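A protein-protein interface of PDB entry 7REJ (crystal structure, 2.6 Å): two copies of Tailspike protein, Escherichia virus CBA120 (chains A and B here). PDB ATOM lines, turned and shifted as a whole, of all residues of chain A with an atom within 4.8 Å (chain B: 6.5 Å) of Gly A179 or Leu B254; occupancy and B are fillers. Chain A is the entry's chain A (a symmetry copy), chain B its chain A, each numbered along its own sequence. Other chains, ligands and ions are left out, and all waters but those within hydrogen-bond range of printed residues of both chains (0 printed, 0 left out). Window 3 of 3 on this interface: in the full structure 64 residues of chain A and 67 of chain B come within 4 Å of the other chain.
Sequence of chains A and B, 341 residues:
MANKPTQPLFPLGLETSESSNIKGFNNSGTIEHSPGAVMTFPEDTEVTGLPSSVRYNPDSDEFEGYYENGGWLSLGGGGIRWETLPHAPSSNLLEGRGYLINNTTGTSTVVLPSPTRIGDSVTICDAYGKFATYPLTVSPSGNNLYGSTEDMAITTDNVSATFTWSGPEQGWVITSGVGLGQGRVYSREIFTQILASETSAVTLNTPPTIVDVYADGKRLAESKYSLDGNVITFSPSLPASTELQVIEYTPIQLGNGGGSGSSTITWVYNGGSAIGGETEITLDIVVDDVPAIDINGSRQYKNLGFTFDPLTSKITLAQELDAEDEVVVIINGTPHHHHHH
The backbone carbonyl oxygen of Gly A179 sits at hydrogen-bond distance from the backbone NH of Asn B256, 3.5 Å away.
Of chain B, only Leu B254 and Asn B256 come within 4 Å of Gly A179.
Leu B254 touches just one residue of chain A: Gly A179.
Printed residues of chain B within 4 Å of Val A178: Ile B174 (3.6 Å) and Leu B180 (3.998 Å).
Printed residues of chain A within 4 Å of Asn B256: Thr A156, Gly A179 and Gly A181.
Asp A157 touches none of the printed residues of chain B.
The nearest printed residue of chain B that does not touch Thr A156 is Leu B254 (4.4 Å).
2 positions are printed for both chains.
Among the printed residues, pairs that only touch across the chains: Thr A156 with Asn B256 (3.6 Å), Val A178 with Ile B174 (3.6 Å), Val A178 with Leu B180 (3.998 Å), Gly A179 with Leu B254 (3.2 Å) and Gly A181 with Asn B256 (3.6 Å).
The side-chain hydroxyl (OH) of Tyr B146 lies within hydrogen-bond range of the backbone NH (N) of Ile B174 (3.0 Å).
Hydrophobic or aromatic side chains of chain A within 4 Å of the printed part of chain B: Val A178.
Of the 12 printed residues of chain B, 4 touch a printed residue of chain A.
Printed residues of chain B that touch a printed residue of chain A: Ile B174, Leu B180, Leu B254 and Asn B256.
Hydrophobic or aromatic side chains of chain B that line the printed part of chain A: Leu B180.
Among the printed residues, no Asp or Glu carboxylate lies within 4 Å of a Lys or Arg side-chain nitrogen of the other chain.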
ATOM      1  N   THR A 156       2.967   7.306   4.842  1.00  0.00           N
ATOM      2  CA  THR A 156       2.346   8.140   3.801  1.00  0.00           C
ATOM      3  C   THR A 156       3.403   8.386   2.749  1.00  0.00           C
ATOM      4  O   THR A 156       4.482   8.848   3.129  1.00  0.00           O
ATOM      5  CB  THR A 156       1.818   9.448   4.384  1.00  0.00           C
ATOM      6  OG1 THR A 156       0.919   9.022   5.398  1.00  0.00           O
ATOM      7  CG2 THR A 156       1.034  10.311   3.418  1.00  0.00           C
ATOM      8  N   ASP A 157       3.150   8.107   1.472  1.00  0.00           N
ATOM      9  CA  ASP A 157       4.236   8.389   0.488  1.00  0.00           C
ATOM     10  C   ASP A 157       4.282   9.887   0.164  1.00  0.00           C
ATOM     11  O   ASP A 157       3.232  10.544   0.342  1.00  0.00           O
ATOM     12  CB  ASP A 157       4.272   7.387  -0.673  1.00  0.00           C
ATOM     13  CG  ASP A 157       3.029   7.290  -1.469  1.00  0.00           C
ATOM     14  OD1 ASP A 157       2.486   8.345  -1.695  1.00  0.00           O
ATOM     15  OD2 ASP A 157       2.651   6.161  -1.834  1.00  0.00           O
ATOM     16  N   VAL A 159       5.823  12.091   1.777  1.00  0.00           N
ATOM     17  CA  VAL A 159       5.927  12.902   3.014  1.00  0.00           C
ATOM     18  C   VAL A 159       7.366  13.371   3.202  1.00  0.00           C
ATOM     19  O   VAL A 159       8.327  12.603   2.932  1.00  0.00           O
ATOM     20  CB  VAL A 159       5.503  12.082   4.234  1.00  0.00           C
ATOM     21  CG1 VAL A 159       6.469  10.964   4.430  1.00  0.00           C
ATOM     22  CG2 VAL A 159       5.452  12.897   5.487  1.00  0.00           C
ATOM     23  N   GLY A 177       7.191  20.081   7.590  1.00  0.00           N
ATOM     24  CA  GLY A 177       6.852  18.861   6.838  1.00  0.00           C
ATOM     25  C   GLY A 177       5.757  19.063   5.829  1.00  0.00           C
ATOM     26  O   GLY A 177       5.253  20.189   5.678  1.00  0.00           O
ATOM     27  N   VAL A 178       5.414  17.981   5.166  1.00  0.00           N
ATOM     28  CA  VAL A 178       4.391  17.980   4.076  1.00  0.00           C
ATOM     29  C   VAL A 178       3.918  16.543   3.958  1.00  0.00           C
ATOM     30  O   VAL A 178       4.766  15.670   4.128  1.00  0.00           O
ATOM     31  CB  VAL A 178       4.985  18.472   2.751  1.00  0.00           C
ATOM     32  CG1 VAL A 178       5.463  19.911   2.882  1.00  0.00           C
ATOM     33  CG2 VAL A 178       6.158  17.588   2.365  1.00  0.00           C
ATOM     34  N   GLY A 179       2.627  16.328   3.682  1.00  0.00           N
ATOM     35  CA  GLY A 179       2.073  14.967   3.500  1.00  0.00           C
ATOM     36  C   GLY A 179       1.802  14.206   4.806  1.00  0.00           C
ATOM     37  O   GLY A 179       1.327  13.063   4.734  1.00  0.00           O
ATOM     38  N   LEU A 180       2.077  14.778   5.976  1.00  0.00           N
ATOM     39  CA  LEU A 180       2.028  13.997   7.227  1.00  0.00           C
ATOM     40  C   LEU A 180       0.591  13.572   7.559  1.00  0.00           C
ATOM     41  O   LEU A 180      -0.245  14.467   7.755  1.00  0.00           O
ATOM     42  CB  LEU A 180       2.602  14.871   8.328  1.00  0.00           C
ATOM     43  CG  LEU A 180       4.118  14.991   8.278  1.00  0.00           C
ATOM     44  CD1 LEU A 180       4.575  16.261   8.996  1.00  0.00           C
ATOM     45  CD2 LEU A 180       4.757  13.733   8.860  1.00  0.00           C
ATOM     46  N   GLY A 181       0.349  12.248   7.614  1.00  0.00           N
ATOM     47  CA  GLY A 181      -0.861  11.637   8.207  1.00  0.00           C
ATOM     48  C   GLY A 181      -0.712  11.125   9.638  1.00  0.00           C
ATOM     49  O   GLY A 181      -0.293  11.885  10.514  1.00  0.00           O
ATOM     50  N   TYR B 146       8.077  15.411  -9.590  1.00  0.00           N
ATOM     51  CA  TYR B 146       7.494  14.137  -9.108  1.00  0.00           C
ATOM     52  C   TYR B 146       7.614  13.081 -10.214  1.00  0.00           C
ATOM     53  O   TYR B 146       6.639  12.419 -10.534  1.00  0.00           O
ATOM     54  CB  TYR B 146       6.056  14.408  -8.679  1.00  0.00           C
ATOM     55  CG  TYR B 146       5.974  15.084  -7.343  1.00  0.00           C
ATOM     56  CD1 TYR B 146       6.291  14.388  -6.191  1.00  0.00           C
ATOM     57  CD2 TYR B 146       5.584  16.410  -7.229  1.00  0.00           C
ATOM     58  CE1 TYR B 146       6.221  14.992  -4.951  1.00  0.00           C
ATOM     59  CE2 TYR B 146       5.508  17.036  -5.995  1.00  0.00           C
ATOM     60  CZ  TYR B 146       5.829  16.318  -4.866  1.00  0.00           C
ATOM     61  OH  TYR B 146       5.753  16.931  -3.662  1.00  0.00           O
ATOM     62  N   MET B 152       2.459  21.516 -13.099  1.00  0.00           N
ATOM     63  CA  MET B 152       1.480  21.251 -12.007  1.00  0.00           C
ATOM     64  C   MET B 152       0.815  22.558 -11.538  1.00  0.00           C
ATOM     65  O   MET B 152       1.459  23.630 -11.476  1.00  0.00           O
ATOM     66  CB  MET B 152       2.187  20.597 -10.827  1.00  0.00           C
ATOM     67  CG  MET B 152       1.289  20.314  -9.665  1.00  0.00           C
ATOM     68  SD  MET B 152       2.176  19.477  -8.351  1.00  0.00           S
ATOM     69  CE  MET B 152       3.001  20.868  -7.598  1.00  0.00           C
ATOM     70  N   ILE B 174       8.201  18.564  -3.282  1.00  0.00           N
ATOM     71  CA  ILE B 174       7.948  19.629  -2.274  1.00  0.00           C
ATOM     72  C   ILE B 174       8.494  19.104  -0.948  1.00  0.00           C
ATOM     73  O   ILE B 174       8.092  18.057  -0.596  1.00  0.00           O
ATOM     74  CB  ILE B 174       6.486  20.082  -2.216  1.00  0.00           C
ATOM     75  CG1 ILE B 174       6.136  20.867  -3.481  1.00  0.00           C
ATOM     76  CG2 ILE B 174       6.253  20.909  -0.965  1.00  0.00           C
ATOM     77  CD1 ILE B 174       4.658  20.849  -3.880  1.00  0.00           C
ATOM     78  N   LEU B 180      -1.344  22.303   1.606  1.00  0.00           N
ATOM     79  CA  LEU B 180      -1.284  21.498   0.371  1.00  0.00           C
ATOM     80  C   LEU B 180      -2.413  20.460   0.330  1.00  0.00           C
ATOM     81  O   LEU B 180      -2.439  19.599   1.224  1.00  0.00           O
ATOM     82  CB  LEU B 180       0.075  20.821   0.339  1.00  0.00           C
ATOM     83  CG  LEU B 180       1.212  21.761  -0.033  1.00  0.00           C
ATOM     84  CD1 LEU B 180       2.544  21.215   0.482  1.00  0.00           C
ATOM     85  CD2 LEU B 180       1.223  21.991  -1.542  1.00  0.00           C
ATOM     86  N   GLY B 181      -3.295  20.564  -0.682  1.00  0.00           N
ATOM     87  CA  GLY B 181      -4.254  19.507  -1.076  1.00  0.00           C
ATOM     88  C   GLY B 181      -3.827  18.627  -2.249  1.00  0.00           C
ATOM     89  O   GLY B 181      -2.737  18.051  -2.210  1.00  0.00           O
ATOM     90  N   GLN B 182      -4.674  18.523  -3.279  1.00  0.00           N
ATOM     91  CA  GLN B 182      -4.360  17.762  -4.519  1.00  0.00           C
ATOM     92  C   GLN B 182      -3.695  18.691  -5.528  1.00  0.00           C
ATOM     93  O   GLN B 182      -4.341  19.676  -6.009  1.00  0.00           O
ATOM     94  CB  GLN B 182      -5.599  17.224  -5.235  1.00  0.00           C
ATOM     95  CG  GLN B 182      -6.300  16.042  -4.587  1.00  0.00           C
ATOM     96  CD  GLN B 182      -7.327  15.454  -5.544  1.00  0.00           C
ATOM     97  OE1 GLN B 182      -7.828  16.132  -6.457  1.00  0.00           O
ATOM     98  NE2 GLN B 182      -7.657  14.176  -5.349  1.00  0.00           N
ATOM     99  N   GLY B 183      -2.449  18.422  -5.861  1.00  0.00           N
ATOM    100  CA  GLY B 183      -1.920  18.975  -7.120  1.00  0.00           C
ATOM    101  C   GLY B 183      -2.775  18.501  -8.292  1.00  0.00           C
ATOM    102  O   GLY B 183      -3.376  17.411  -8.212  1.00  0.00           O
ATOM    103  N   ILE B 252      -2.437  14.777  -7.801  1.00  0.00           N
ATOM    104  CA  ILE B 252      -1.140  14.392  -7.196  1.00  0.00           C
ATOM    105  C   ILE B 252      -1.361  14.573  -5.689  1.00  0.00           C
ATOM    106  O   ILE B 252      -1.586  15.695  -5.245  1.00  0.00           O
ATOM    107  CB  ILE B 252      -0.015  15.186  -7.877  1.00  0.00           C
ATOM    108  CG1 ILE B 252       1.283  15.143  -7.085  1.00  0.00           C
ATOM    109  CG2 ILE B 252      -0.469  16.604  -8.125  1.00  0.00           C
ATOM    110  CD1 ILE B 252       2.151  13.982  -7.450  1.00  0.00           C
ATOM    111  N   GLN B 253      -1.300  13.488  -4.930  1.00  0.00           N
ATOM    112  CA  GLN B 253      -1.749  13.519  -3.522  1.00  0.00           C
ATOM    113  C   GLN B 253      -0.576  13.883  -2.614  1.00  0.00           C
ATOM    114  O   GLN B 253       0.466  13.199  -2.621  1.00  0.00           O
ATOM    115  CB  GLN B 253      -2.377  12.194  -3.082  1.00  0.00           C
ATOM    116  CG  GLN B 253      -3.051  12.284  -1.712  1.00  0.00           C
ATOM    117  CD  GLN B 253      -3.937  13.506  -1.602  1.00  0.00           C
ATOM    118  OE1 GLN B 253      -4.924  13.646  -2.334  1.00  0.00           O
ATOM    119  NE2 GLN B 253      -3.598  14.406  -0.688  1.00  0.00           N
ATOM    120  N   LEU B 254      -0.761  14.944  -1.853  1.00  0.00           N
ATOM    121  CA  LEU B 254       0.254  15.388  -0.863  1.00  0.00           C
ATOM    122  C   LEU B 254      -0.288  15.018   0.526  1.00  0.00           C
ATOM    123  O   LEU B 254       0.248  14.013   1.111  1.00  0.00           O
ATOM    124  CB  LEU B 254       0.493  16.881  -1.096  1.00  0.00           C
ATOM    125  CG  LEU B 254       0.483  17.231  -2.591  1.00  0.00           C
ATOM    126  CD1 LEU B 254       0.489  18.724  -2.869  1.00  0.00           C
ATOM    127  CD2 LEU B 254       1.653  16.576  -3.292  1.00  0.00           C
ATOM    128  N   GLY B 255      -1.287  15.781   1.016  1.00  0.00           N
ATOM    129  CA  GLY B 255      -1.916  15.612   2.343  1.00  0.00           C
ATOM    130  C   GLY B 255      -2.390  14.181   2.575  1.00  0.00           C
ATOM    131  O   GLY B 255      -3.183  13.695   1.745  1.00  0.00           O
ATOM    132  N   ASN B 256      -1.927  13.528   3.656  1.00  0.00           N
ATOM    133  CA  ASN B 256      -2.343  12.151   4.067  1.00  0.00           C
ATOM    134  C   ASN B 256      -2.353  11.230   2.837  1.00  0.00           C
ATOM    135  O   ASN B 256      -2.671  10.037   3.006  1.00  0.00           O
ATOM    136  CB  ASN B 256      -3.706  12.162   4.773  1.00  0.00           C
ATOM    137  CG  ASN B 256      -4.128  10.822   5.352  1.00  0.00           C
ATOM    138  OD1 ASN B 256      -3.360  10.177   6.057  1.00  0.00           O
ATOM    139  ND2 ASN B 256      -5.349  10.393   5.063  1.00  0.00           N
